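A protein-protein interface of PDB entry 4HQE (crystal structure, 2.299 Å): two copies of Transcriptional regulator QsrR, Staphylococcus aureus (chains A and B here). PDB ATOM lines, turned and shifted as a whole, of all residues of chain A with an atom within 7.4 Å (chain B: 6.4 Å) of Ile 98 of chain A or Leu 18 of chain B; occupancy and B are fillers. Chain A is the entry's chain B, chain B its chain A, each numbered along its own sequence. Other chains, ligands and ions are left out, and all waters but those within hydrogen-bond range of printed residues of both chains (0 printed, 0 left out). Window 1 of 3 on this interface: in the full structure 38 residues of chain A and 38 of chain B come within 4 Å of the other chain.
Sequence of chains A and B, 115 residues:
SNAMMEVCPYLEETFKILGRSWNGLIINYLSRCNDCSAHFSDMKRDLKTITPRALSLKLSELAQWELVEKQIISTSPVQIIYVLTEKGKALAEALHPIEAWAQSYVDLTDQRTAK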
ATOM      1  N   PHE A  15       7.287 -18.994 -12.416  1.00  0.00           N
ATOM      2  CA  PHE A  15       6.590 -20.267 -12.243  1.00  0.00           C
ATOM      3  C   PHE A  15       7.350 -21.466 -12.822  1.00  0.00           C
ATOM      4  O   PHE A  15       7.071 -22.616 -12.465  1.00  0.00           O
ATOM      5  CB  PHE A  15       5.148 -20.184 -12.729  1.00  0.00           C
ATOM      6  CG  PHE A  15       4.204 -19.677 -11.672  1.00  0.00           C
ATOM      7  CD1 PHE A  15       3.731 -20.535 -10.678  1.00  0.00           C
ATOM      8  CD2 PHE A  15       3.824 -18.341 -11.641  1.00  0.00           C
ATOM      9  CE1 PHE A  15       2.875 -20.068  -9.685  1.00  0.00           C
ATOM     10  CE2 PHE A  15       2.965 -17.871 -10.650  1.00  0.00           C
ATOM     11  CZ  PHE A  15       2.493 -18.736  -9.674  1.00  0.00           C
ATOM     12  N   ILE A  17      10.112 -22.167 -11.785  1.00  0.00           N
ATOM     13  CA  ILE A  17      10.637 -22.775 -10.559  1.00  0.00           C
ATOM     14  C   ILE A  17       9.525 -23.046  -9.555  1.00  0.00           C
ATOM     15  O   ILE A  17       9.486 -24.112  -8.943  1.00  0.00           O
ATOM     16  CB  ILE A  17      11.700 -21.915  -9.836  1.00  0.00           C
ATOM     17  CG1 ILE A  17      11.945 -20.608 -10.573  1.00  0.00           C
ATOM     18  CG2 ILE A  17      13.011 -22.717  -9.662  1.00  0.00           C
ATOM     19  CD1 ILE A  17      12.772 -19.611  -9.774  1.00  0.00           C
ATOM     20  N   LEU A  18       8.643 -22.068  -9.371  1.00  0.00           N
ATOM     21  CA  LEU A  18       7.567 -22.201  -8.400  1.00  0.00           C
ATOM     22  C   LEU A  18       6.535 -23.233  -8.850  1.00  0.00           C
ATOM     23  O   LEU A  18       5.955 -23.925  -8.018  1.00  0.00           O
ATOM     24  CB  LEU A  18       6.884 -20.856  -8.150  1.00  0.00           C
ATOM     25  CG  LEU A  18       7.474 -19.941  -7.074  1.00  0.00           C
ATOM     26  CD1 LEU A  18       6.455 -18.852  -6.674  1.00  0.00           C
ATOM     27  CD2 LEU A  18       7.928 -20.759  -5.861  1.00  0.00           C
ATOM     28  N   GLY A  19       6.320 -23.342 -10.162  1.00  0.00           N
ATOM     29  CA  GLY A  19       5.312 -24.254 -10.696  1.00  0.00           C
ATOM     30  C   GLY A  19       5.846 -25.653 -10.974  1.00  0.00           C
ATOM     31  O   GLY A  19       5.404 -26.317 -11.929  1.00  0.00           O
ATOM     32  N   ARG A  20       6.798 -26.087 -10.146  1.00  0.00           N
ATOM     33  CA  ARG A  20       7.360 -27.431 -10.202  1.00  0.00           C
ATOM     34  C   ARG A  20       7.344 -27.994  -8.787  1.00  0.00           C
ATOM     35  O   ARG A  20       7.062 -27.265  -7.827  1.00  0.00           O
ATOM     36  CB  ARG A  20       8.804 -27.400 -10.714  1.00  0.00           C
ATOM     37  CG  ARG A  20       9.020 -26.549 -11.948  1.00  0.00           C
ATOM     38  CD  ARG A  20       9.056 -27.421 -13.188  1.00  0.00           C
ATOM     39  NE  ARG A  20       7.800 -28.147 -13.351  1.00  0.00           N
ATOM     40  CZ  ARG A  20       6.839 -27.791 -14.203  1.00  0.00           C
ATOM     41  NH1 ARG A  20       7.001 -26.725 -14.991  1.00  0.00           N
ATOM     42  NH2 ARG A  20       5.713 -28.501 -14.273  1.00  0.00           N
ATOM     43  N   SER A  21       7.662 -29.277  -8.647  1.00  0.00           N
ATOM     44  CA  SER A  21       7.674 -29.903  -7.327  1.00  0.00           C
ATOM     45  C   SER A  21       8.761 -29.319  -6.394  1.00  0.00           C
ATOM     46  O   SER A  21       9.865 -28.982  -6.839  1.00  0.00           O
ATOM     47  CB  SER A  21       7.857 -31.425  -7.444  1.00  0.00           C
ATOM     48  OG  SER A  21       9.092 -31.742  -8.083  1.00  0.00           O
ATOM     49  N   GLU A  93       9.982 -14.321   1.445  1.00  0.00           N
ATOM     50  CA  GLU A  93       9.107 -13.306   2.020  1.00  0.00           C
ATOM     51  C   GLU A  93       7.829 -13.159   1.189  1.00  0.00           C
ATOM     52  O   GLU A  93       6.728 -13.075   1.744  1.00  0.00           O
ATOM     53  CB  GLU A  93       9.832 -11.959   2.144  1.00  0.00           C
ATOM     54  CG  GLU A  93      10.631 -11.804   3.435  1.00  0.00           C
ATOM     55  CD  GLU A  93       9.758 -11.915   4.693  1.00  0.00           C
ATOM     56  OE1 GLU A  93       8.791 -11.124   4.836  1.00  0.00           O
ATOM     57  OE2 GLU A  93      10.044 -12.795   5.542  1.00  0.00           O
ATOM     58  N   ALA A  94       7.993 -13.151  -0.137  1.00  0.00           N
ATOM     59  CA  ALA A  94       6.874 -13.058  -1.077  1.00  0.00           C
ATOM     60  C   ALA A  94       5.859 -14.217  -0.970  1.00  0.00           C
ATOM     61  O   ALA A  94       4.779 -14.137  -1.556  1.00  0.00           O
ATOM     62  CB  ALA A  94       7.400 -12.939  -2.507  1.00  0.00           C
ATOM     63  N   LEU A  95       6.195 -15.278  -0.228  1.00  0.00           N
ATOM     64  CA  LEU A  95       5.290 -16.423  -0.086  1.00  0.00           C
ATOM     65  C   LEU A  95       4.422 -16.377   1.180  1.00  0.00           C
ATOM     66  O   LEU A  95       3.477 -17.156   1.306  1.00  0.00           O
ATOM     67  CB  LEU A  95       6.053 -17.758  -0.116  1.00  0.00           C
ATOM     68  CG  LEU A  95       6.940 -18.193  -1.293  1.00  0.00           C
ATOM     69  CD1 LEU A  95       7.571 -19.544  -0.977  1.00  0.00           C
ATOM     70  CD2 LEU A  95       6.177 -18.282  -2.600  1.00  0.00           C
ATOM     71  N   HIS A  96       4.738 -15.496   2.125  1.00  0.00           N
ATOM     72  CA  HIS A  96       3.921 -15.406   3.343  1.00  0.00           C
ATOM     73  C   HIS A  96       2.406 -15.322   3.098  1.00  0.00           C
ATOM     74  O   HIS A  96       1.649 -16.075   3.709  1.00  0.00           O
ATOM     75  CB  HIS A  96       4.420 -14.297   4.292  1.00  0.00           C
ATOM     76  CG  HIS A  96       5.715 -14.635   4.963  1.00  0.00           C
ATOM     77  ND1 HIS A  96       5.995 -15.903   5.424  1.00  0.00           N
ATOM     78  CD2 HIS A  96       6.821 -13.890   5.212  1.00  0.00           C
ATOM     79  CE1 HIS A  96       7.213 -15.924   5.946  1.00  0.00           C
ATOM     80  NE2 HIS A  96       7.732 -14.715   5.824  1.00  0.00           N
ATOM     81  N   PRO A  97       1.954 -14.435   2.189  1.00  0.00           N
ATOM     82  CA  PRO A  97       0.488 -14.357   2.010  1.00  0.00           C
ATOM     83  C   PRO A  97      -0.144 -15.629   1.409  1.00  0.00           C
ATOM     84  O   PRO A  97      -1.349 -15.897   1.605  1.00  0.00           O
ATOM     85  CB  PRO A  97       0.299 -13.147   1.073  1.00  0.00           C
ATOM     86  CG  PRO A  97       1.639 -12.946   0.411  1.00  0.00           C
ATOM     87  CD  PRO A  97       2.682 -13.446   1.369  1.00  0.00           C
ATOM     88  N   ILE A  98       0.659 -16.390   0.674  1.00  0.00           N
ATOM     89  CA  ILE A  98       0.276 -17.738   0.251  1.00  0.00           C
ATOM     90  C   ILE A  98       0.039 -18.640   1.472  1.00  0.00           C
ATOM     91  O   ILE A  98      -0.985 -19.347   1.550  1.00  0.00           O
ATOM     92  CB  ILE A  98       1.352 -18.347  -0.664  1.00  0.00           C
ATOM     93  CG1 ILE A  98       1.521 -17.459  -1.900  1.00  0.00           C
ATOM     94  CG2 ILE A  98       1.004 -19.776  -1.049  1.00  0.00           C
ATOM     95  CD1 ILE A  98       2.315 -18.081  -3.000  1.00  0.00           C
ATOM     96  N   GLU A  99       0.980 -18.600   2.419  1.00  0.00           N
ATOM     97  CA  GLU A  99       0.823 -19.285   3.697  1.00  0.00           C
ATOM     98  C   GLU A  99      -0.458 -18.862   4.396  1.00  0.00           C
ATOM     99  O   GLU A  99      -1.235 -19.708   4.853  1.00  0.00           O
ATOM    100  CB  GLU A  99       2.000 -18.983   4.620  1.00  0.00           C
ATOM    101  CG  GLU A  99       3.151 -19.952   4.493  1.00  0.00           C
ATOM    102  CD  GLU A  99       4.139 -19.800   5.631  1.00  0.00           C
ATOM    103  OE1 GLU A  99       5.173 -19.116   5.422  1.00  0.00           O
ATOM    104  OE2 GLU A  99       3.859 -20.355   6.726  1.00  0.00           O
ATOM    105  N   ALA A 100      -0.662 -17.548   4.478  1.00  0.00           N
ATOM    106  CA  ALA A 100      -1.861 -16.975   5.085  1.00  0.00           C
ATOM    107  C   ALA A 100      -3.124 -17.483   4.376  1.00  0.00           C
ATOM    108  O   ALA A 100      -4.060 -17.956   5.029  1.00  0.00           O
ATOM    109  CB  ALA A 100      -1.791 -15.459   5.050  1.00  0.00           C
ATOM    110  N   TRP A 101      -3.141 -17.393   3.048  1.00  0.00           N
ATOM    111  CA  TRP A 101      -4.245 -17.926   2.246  1.00  0.00           C
ATOM    112  C   TRP A 101      -4.502 -19.413   2.557  1.00  0.00           C
ATOM    113  O   TRP A 101      -5.647 -19.819   2.772  1.00  0.00           O
ATOM    114  CB  TRP A 101      -3.952 -17.758   0.755  1.00  0.00           C
ATOM    115  CG  TRP A 101      -5.050 -18.304  -0.105  1.00  0.00           C
ATOM    116  CD1 TRP A 101      -6.181 -17.651  -0.504  1.00  0.00           C
ATOM    117  CD2 TRP A 101      -5.137 -19.632  -0.656  1.00  0.00           C
ATOM    118  NE1 TRP A 101      -6.967 -18.485  -1.266  1.00  0.00           N
ATOM    119  CE2 TRP A 101      -6.347 -19.703  -1.382  1.00  0.00           C
ATOM    120  CE3 TRP A 101      -4.306 -20.762  -0.604  1.00  0.00           C
ATOM    121  CZ2 TRP A 101      -6.755 -20.870  -2.057  1.00  0.00           C
ATOM    122  CZ3 TRP A 101      -4.709 -21.920  -1.278  1.00  0.00           C
ATOM    123  CH2 TRP A 101      -5.928 -21.964  -1.989  1.00  0.00           C
ATOM    124  N   ALA A 102      -3.419 -20.197   2.580  1.00  0.00           N
ATOM    125  CA  ALA A 102      -3.443 -21.628   2.901  1.00  0.00           C
ATOM    126  C   ALA A 102      -4.109 -21.966   4.242  1.00  0.00           C
ATOM    127  O   ALA A 102      -4.837 -22.954   4.351  1.00  0.00           O
ATOM    128  CB  ALA A 102      -2.020 -22.182   2.883  1.00  0.00           C
ATOM    129  N   GLN A 103      -3.844 -21.159   5.265  1.00  0.00           N
ATOM    130  CA  GLN A 103      -4.392 -21.417   6.591  1.00  0.00           C
ATOM    131  C   GLN A 103      -5.822 -20.897   6.705  1.00  0.00           C
ATOM    132  O   GLN A 103      -6.584 -21.341   7.571  1.00  0.00           O
ATOM    133  CB  GLN A 103      -3.486 -20.801   7.665  1.00  0.00           C
ATOM    134  CG  GLN A 103      -2.040 -21.320   7.596  1.00  0.00           C
ATOM    135  CD  GLN A 103      -1.089 -20.558   8.515  1.00  0.00           C
ATOM    136  OE1 GLN A 103      -1.388 -20.344   9.688  1.00  0.00           O
ATOM    137  NE2 GLN A 103       0.067 -20.149   7.978  1.00  0.00           N
ATOM    138  N   SER A 104      -6.192 -19.969   5.830  1.00  0.00           N
ATOM    139  CA  SER A 104      -7.560 -19.464   5.814  1.00  0.00           C
ATOM    140  C   SER A 104      -8.522 -20.336   5.000  1.00  0.00           C
ATOM    141  O   SER A 104      -9.664 -20.534   5.409  1.00  0.00           O
ATOM    142  CB  SER A 104      -7.603 -18.019   5.294  1.00  0.00           C
ATOM    143  OG  SER A 104      -7.192 -17.101   6.293  1.00  0.00           O
ATOM    144  N   VAL A 106      -7.734 -23.557   2.965  1.00  0.00           N
ATOM    145  CA  VAL A 106      -7.510 -24.967   2.690  1.00  0.00           C
ATOM    146  C   VAL A 106      -8.065 -25.855   3.803  1.00  0.00           C
ATOM    147  O   VAL A 106      -7.819 -25.612   4.990  1.00  0.00           O
ATOM    148  CB  VAL A 106      -6.012 -25.287   2.489  1.00  0.00           C
ATOM    149  CG1 VAL A 106      -5.786 -26.806   2.357  1.00  0.00           C
ATOM    150  CG2 VAL A 106      -5.460 -24.553   1.272  1.00  0.00           C
ATOM    151  N   TYR B  10      -0.805 -27.027   5.399  1.00  0.00           N
ATOM    152  CA  TYR B  10      -1.647 -26.186   4.545  1.00  0.00           C
ATOM    153  C   TYR B  10      -0.840 -25.602   3.398  1.00  0.00           C
ATOM    154  O   TYR B  10      -1.281 -25.600   2.250  1.00  0.00           O
ATOM    155  CB  TYR B  10      -2.270 -25.060   5.350  1.00  0.00           C
ATOM    156  CG  TYR B  10      -3.195 -25.575   6.406  1.00  0.00           C
ATOM    157  CD1 TYR B  10      -4.555 -25.699   6.153  1.00  0.00           C
ATOM    158  CD2 TYR B  10      -2.714 -25.945   7.659  1.00  0.00           C
ATOM    159  CE1 TYR B  10      -5.424 -26.173   7.112  1.00  0.00           C
ATOM    160  CE2 TYR B  10      -3.581 -26.428   8.643  1.00  0.00           C
ATOM    161  CZ  TYR B  10      -4.940 -26.540   8.353  1.00  0.00           C
ATOM    162  OH  TYR B  10      -5.826 -27.021   9.295  1.00  0.00           O
ATOM    163  N   LEU B  11       0.343 -25.090   3.717  1.00  0.00           N
ATOM    164  CA  LEU B  11       1.240 -24.621   2.675  1.00  0.00           C
ATOM    165  C   LEU B  11       1.536 -25.780   1.739  1.00  0.00           C
ATOM    166  O   LEU B  11       1.472 -25.640   0.523  1.00  0.00           O
ATOM    167  CB  LEU B  11       2.554 -24.084   3.262  1.00  0.00           C
ATOM    168  CG  LEU B  11       3.507 -23.609   2.164  1.00  0.00           C
ATOM    169  CD1 LEU B  11       2.848 -22.492   1.357  1.00  0.00           C
ATOM    170  CD2 LEU B  11       4.859 -23.153   2.756  1.00  0.00           C
ATOM    171  N   GLU B  13      -0.162 -28.455   1.041  1.00  0.00           N
ATOM    172  CA  GLU B  13      -1.342 -28.699   0.235  1.00  0.00           C
ATOM    173  C   GLU B  13      -1.487 -27.633  -0.856  1.00  0.00           C
ATOM    174  O   GLU B  13      -1.810 -27.951  -2.008  1.00  0.00           O
ATOM    175  CB  GLU B  13      -2.577 -28.733   1.137  1.00  0.00           C
ATOM    176  CG  GLU B  13      -3.823 -29.312   0.487  1.00  0.00           C
ATOM    177  CD  GLU B  13      -3.848 -30.843   0.497  1.00  0.00           C
ATOM    178  OE1 GLU B  13      -4.937 -31.415   0.240  1.00  0.00           O
ATOM    179  OE2 GLU B  13      -2.789 -31.472   0.762  1.00  0.00           O
ATOM    180  N   THR B  14      -1.218 -26.377  -0.510  1.00  0.00           N
ATOM    181  CA  THR B  14      -1.276 -25.302  -1.506  1.00  0.00           C
ATOM    182  C   THR B  14      -0.331 -25.541  -2.685  1.00  0.00           C
ATOM    183  O   THR B  14      -0.704 -25.328  -3.845  1.00  0.00           O
ATOM    184  CB  THR B  14      -0.992 -23.924  -0.896  1.00  0.00           C
ATOM    185  OG1 THR B  14      -1.943 -23.665   0.141  1.00  0.00           O
ATOM    186  CG2 THR B  14      -1.125 -22.840  -1.958  1.00  0.00           C
ATOM    187  N   PHE B  15       0.878 -26.015  -2.399  1.00  0.00           N
ATOM    188  CA  PHE B  15       1.821 -26.274  -3.481  1.00  0.00           C
ATOM    189  C   PHE B  15       1.451 -27.453  -4.368  1.00  0.00           C
ATOM    190  O   PHE B  15       1.991 -27.601  -5.458  1.00  0.00           O
ATOM    191  CB  PHE B  15       3.270 -26.340  -2.979  1.00  0.00           C
ATOM    192  CG  PHE B  15       3.933 -25.003  -2.982  1.00  0.00           C
ATOM    193  CD1 PHE B  15       4.338 -24.425  -4.177  1.00  0.00           C
ATOM    194  CD2 PHE B  15       4.071 -24.276  -1.810  1.00  0.00           C
ATOM    195  CE1 PHE B  15       4.915 -23.163  -4.193  1.00  0.00           C
ATOM    196  CE2 PHE B  15       4.642 -23.009  -1.825  1.00  0.00           C
ATOM    197  CZ  PHE B  15       5.065 -22.460  -3.014  1.00  0.00           C
ATOM    198  N   LYS B  16       0.504 -28.276  -3.932  1.00  0.00           N
ATOM    199  CA  LYS B  16      -0.019 -29.291  -4.839  1.00  0.00           C
ATOM    200  C   LYS B  16      -0.703 -28.649  -6.064  1.00  0.00           C
ATOM    201  O   LYS B  16      -0.707 -29.246  -7.139  1.00  0.00           O
ATOM    202  CB  LYS B  16      -0.959 -30.254  -4.109  1.00  0.00           C
ATOM    203  CG  LYS B  16      -0.290 -30.976  -2.946  1.00  0.00           C
ATOM    204  CD  LYS B  16      -0.826 -32.395  -2.763  1.00  0.00           C
ATOM    205  CE  LYS B  16      -0.220 -33.054  -1.517  1.00  0.00           C
ATOM    206  NZ  LYS B  16       1.283 -33.067  -1.524  1.00  0.00           N
ATOM    207  N   ILE B  17      -1.272 -27.446  -5.909  1.00  0.00           N
ATOM    208  CA  ILE B  17      -1.818 -26.720  -7.079  1.00  0.00           C
ATOM    209  C   ILE B  17      -0.802 -25.781  -7.705  1.00  0.00           C
ATOM    210  O   ILE B  17      -0.576 -25.805  -8.915  1.00  0.00           O
ATOM    211  CB  ILE B  17      -3.046 -25.844  -6.751  1.00  0.00           C
ATOM    212  CG1 ILE B  17      -3.435 -25.992  -5.291  1.00  0.00           C
ATOM    213  CG2 ILE B  17      -4.218 -26.194  -7.694  1.00  0.00           C
ATOM    214  CD1 ILE B  17      -3.935 -24.728  -4.674  1.00  0.00           C
ATOM    215  N   LEU B  18      -0.214 -24.927  -6.870  1.00  0.00           N
ATOM    216  CA  LEU B  18       0.739 -23.922  -7.335  1.00  0.00           C
ATOM    217  C   LEU B  18       2.031 -24.536  -7.867  1.00  0.00           C
ATOM    218  O   LEU B  18       2.651 -23.982  -8.784  1.00  0.00           O
ATOM    219  CB  LEU B  18       1.061 -22.950  -6.209  1.00  0.00           C
ATOM    220  CG  LEU B  18      -0.036 -21.929  -5.947  1.00  0.00           C
ATOM    221  CD1 LEU B  18       0.396 -20.959  -4.843  1.00  0.00           C
ATOM    222  CD2 LEU B  18      -0.352 -21.195  -7.259  1.00  0.00           C
ATOM    223  N   GLY B  19       2.418 -25.685  -7.307  1.00  0.00           N
ATOM    224  CA  GLY B  19       3.688 -26.316  -7.648  1.00  0.00           C
ATOM    225  C   GLY B  19       3.538 -27.239  -8.832  1.00  0.00           C
ATOM    226  O   GLY B  19       4.226 -28.264  -8.921  1.00  0.00           O
ATOM    227  N   ARG B  20       2.613 -26.887  -9.726  1.00  0.00           N
ATOM    228  CA  ARG B  20       2.428 -27.599 -10.986  1.00  0.00           C
ATOM    229  C   ARG B  20       2.349 -26.572 -12.100  1.00  0.00           C
ATOM    230  O   ARG B  20       2.123 -25.381 -11.845  1.00  0.00           O
ATOM    231  CB  ARG B  20       1.155 -28.466 -10.956  1.00  0.00           C
ATOM    232  CG  ARG B  20       1.073 -29.346  -9.711  1.00  0.00           C
ATOM    233  CD  ARG B  20       1.802 -30.692  -9.852  1.00  0.00           C
ATOM    234  NE  ARG B  20       2.799 -30.739 -10.925  1.00  0.00           N
ATOM    235  CZ  ARG B  20       4.094 -31.012 -10.745  1.00  0.00           C
ATOM    236  NH1 ARG B  20       4.549 -31.262  -9.520  1.00  0.00           N
ATOM    237  NH2 ARG B  20       4.937 -31.039 -11.789  1.00  0.00           N
ATOM    238  N   SER B  21       2.541 -27.038 -13.328  1.00  0.00           N
ATOM    239  CA  SER B  21       2.524 -26.179 -14.494  1.00  0.00           C
ATOM    240  C   SER B  21       1.161 -25.489 -14.644  1.00  0.00           C
ATOM    241  O   SER B  21       0.107 -26.072 -14.294  1.00  0.00           O
ATOM    242  CB  SER B  21       2.842 -27.011 -15.737  1.00  0.00           C
ATOM    243  OG  SER B  21       1.871 -28.031 -15.884  1.00  0.00           O
ATOM    244  N   ASN B  23      -1.062 -23.580 -13.294  1.00  0.00           N
ATOM    245  CA  ASN B  23      -2.138 -23.218 -12.360  1.00  0.00           C
ATOM    246  C   ASN B  23      -2.073 -21.780 -11.834  1.00  0.00           C
ATOM    247  O   ASN B  23      -3.100 -21.084 -11.788  1.00  0.00           O
ATOM    248  CB  ASN B  23      -2.244 -24.224 -11.209  1.00  0.00           C
ATOM    249  CG  ASN B  23      -2.776 -25.576 -11.665  1.00  0.00           C
ATOM    250  OD1 ASN B  23      -3.530 -25.659 -12.636  1.00  0.00           O
ATOM    251  ND2 ASN B  23      -2.388 -26.639 -10.965  1.00  0.00           N
ATOM    252  N   GLY B  24      -0.879 -21.337 -11.443  1.00  0.00           N
ATOM    253  CA  GLY B  24      -0.692 -19.963 -10.996  1.00  0.00           C
ATOM    254  C   GLY B  24      -0.950 -18.962 -12.108  1.00  0.00           C
ATOM    255  O   GLY B  24      -1.565 -17.916 -11.877  1.00  0.00           O
ATOM    256  N   LEU B  25      -0.492 -19.288 -13.314  1.00  0.00           N
ATOM    257  CA  LEU B  25      -0.699 -18.417 -14.471  1.00  0.00           C
ATOM    258  C   LEU B  25      -2.184 -18.293 -14.843  1.00  0.00           C
ATOM    259  O   LEU B  25      -2.659 -17.198 -15.172  1.00  0.00           O
ATOM    260  CB  LEU B  25       0.118 -18.913 -15.669  1.00  0.00           C
ATOM    261  CG  LEU B  25       1.629 -18.869 -15.515  1.00  0.00           C
ATOM    262  CD1 LEU B  25       2.315 -19.162 -16.867  1.00  0.00           C
ATOM    263  CD2 LEU B  25       2.080 -17.517 -14.945  1.00  0.00           C
ATOM    264  N   ILE B  27      -4.817 -18.710 -12.791  1.00  0.00           N
ATOM    265  CA  ILE B  27      -5.517 -18.015 -11.703  1.00  0.00           C
ATOM    266  C   ILE B  27      -5.253 -16.500 -11.760  1.00  0.00           C
ATOM    267  O   ILE B  27      -6.147 -15.664 -11.518  1.00  0.00           O
ATOM    268  CB  ILE B  27      -5.066 -18.559 -10.335  1.00  0.00           C
ATOM    269  CG1 ILE B  27      -5.653 -19.951 -10.103  1.00  0.00           C
ATOM    270  CG2 ILE B  27      -5.476 -17.619  -9.201  1.00  0.00           C
ATOM    271  CD1 ILE B  27      -4.909 -20.742  -9.047  1.00  0.00           C
ATOM    272  N   LEU B  91      -6.612 -16.266  -3.700  1.00  0.00           N
ATOM    273  CA  LEU B  91      -5.325 -16.836  -4.102  1.00  0.00           C
ATOM    274  C   LEU B  91      -4.578 -15.905  -5.065  1.00  0.00           C
ATOM    275  O   LEU B  91      -3.372 -15.677  -4.917  1.00  0.00           O
ATOM    276  CB  LEU B  91      -5.510 -18.210  -4.757  1.00  0.00           C
ATOM    277  CG  LEU B  91      -4.561 -19.356  -4.391  1.00  0.00           C
ATOM    278  CD1 LEU B  91      -4.466 -20.329  -5.551  1.00  0.00           C
ATOM    279  CD2 LEU B  91      -3.143 -18.904  -3.909  1.00  0.00           C
ATOM    280  N   ALA B  94      -2.981 -13.129  -3.323  1.00  0.00           N
ATOM    281  CA  ALA B  94      -1.850 -13.607  -2.543  1.00  0.00           C
ATOM    282  C   ALA B  94      -0.624 -13.870  -3.420  1.00  0.00           C
ATOM    283  O   ALA B  94       0.448 -14.189  -2.907  1.00  0.00           O
ATOM    284  CB  ALA B  94      -2.245 -14.859  -1.740  1.00  0.00           C
ATOM    285  N   LEU B  95      -0.779 -13.701  -4.734  1.00  0.00           N
ATOM    286  CA  LEU B  95       0.309 -13.909  -5.683  1.00  0.00           C
ATOM    287  C   LEU B  95       0.971 -12.616  -6.127  1.00  0.00           C
ATOM    288  O   LEU B  95       1.985 -12.638  -6.826  1.00  0.00           O
ATOM    289  CB  LEU B  95      -0.206 -14.644  -6.922  1.00  0.00           C
ATOM    290  CG  LEU B  95      -0.666 -16.072  -6.662  1.00  0.00           C
ATOM    291  CD1 LEU B  95      -1.371 -16.658  -7.881  1.00  0.00           C
ATOM    292  CD2 LEU B  95       0.551 -16.904  -6.285  1.00  0.00           C
ATOM    293  N   ILE B  98       4.705 -12.086  -5.207  1.00  0.00           N
ATOM    294  CA  ILE B  98       5.558 -12.913  -6.064  1.00  0.00           C
ATOM    295  C   ILE B  98       5.853 -12.189  -7.370  1.00  0.00           C
ATOM    296  O   ILE B  98       6.967 -12.253  -7.899  1.00  0.00           O
ATOM    297  CB  ILE B  98       4.886 -14.265  -6.392  1.00  0.00           C
ATOM    298  CG1 ILE B  98       4.905 -15.189  -5.174  1.00  0.00           C
ATOM    299  CG2 ILE B  98       5.547 -14.939  -7.574  1.00  0.00           C
ATOM    300  CD1 ILE B  98       3.664 -15.045  -4.298  1.00  0.00           C
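O of Tyr 10 of chain B lies within hydrogen-bond range of OG1 of Thr 14 of chain B, at 2.9 Å.
Of the 19 printed residues of chain B, 14 touch a printed residue of chain A. Printed residues of chain A that touch a printed residue of chain B: Phe 15, Leu 18, Gly 19, Arg 20, Ser 21, Ala 94, Pro 97, Ile 98, Trp 101, Ala 102 and Val 106. Among the printed residues, 28 pairs touch across the chains.
Leu 18 of chain A touches its own counterpart, Leu 18 of chain B. Leu 18 of chain A touches Gly 19 of chain B, and with the chains exchanged Gly 19 of chain A touches Leu 18 of chain B. Gly 19 of chain A touches Arg 20 of chain B, and with the chains exchanged Arg 20 of chain A touches Gly 19 of chain B. Ile 98 of chain A touches Leu 18 of chain B, but with the chains exchanged Leu 18 of chain A does not touch Ile 98 of chain B (4.1 Å).
Phe 15 of chain A touches Leu 25 of chain B (CD2 to CD2, 3.8 Å). Arg 20 of chain A touches Ser 21 of chain B. Gly 19 of chain B touches Ser 21 of chain A (O to N, 3.6 Å). N of Ser 21 of chain A touches NH1 of Arg 20 of chain B (3.8 Å). CG2 of Ile 98 of chain A touches CG2 of Thr 14 of chain B, at 3.8 Å. CD2 of Leu 95 of chain B touches CD1 of Ile 98 of chain A, at 3.9 Å. Thr 14 of chain B touches Trp 101 of chain A (OG1 to CZ3, 3.6 Å). CB of Ala 102 of chain A touches OG1 of Thr 14 of chain B, at 3.1 Å. Val 106 of chain A touches Tyr 10 of chain B (O to CE1, 3.2 Å). OG1 of Thr 14 of chain B touches CG2 of Val 106 of chain A, at 3.8 Å.
Of chain B, only Thr 14 (3.8 Å), Leu 18 (3.9 Å), Ala 94 (3.6 Å), Leu 95 (3.9 Å) and Ile 98 (3.6 Å) come within 4 Å of Ile 98 of chain A. Printed residues of chain A within 4 Å of Gly 24 of chain B: Phe 15. Of the printed residues of chain A, Leu 25 of chain B touches Phe 15. Printed residues of chain A within 4 Å of Ala 94 of chain B: Pro 97 and Ile 98.
N of Ser 21 of chain B is in hydrogen-bond range of O of Gly 19 of chain A, 3.3 Å away. The backbone carbonyl oxygen of Leu 18 of chain A sits close to the backbone carbonyl oxygen of Leu 18 of chain B, 3.4 Å away. The backbone carbonyl oxygen of Gly 19 of chain A lies close to the backbone carbonyl oxygen of Arg 20 of chain B, at 3.4 Å. The backbone carbonyl oxygen of Arg 20 of chain A lies close to the backbone carbonyl oxygen of Gly 19 of chain B, at 3.2 Å. The indole nitrogen (NE1) of Trp 101 of chain A lies close to the backbone NH (N) of Leu 91 of chain B (3.3 Å).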
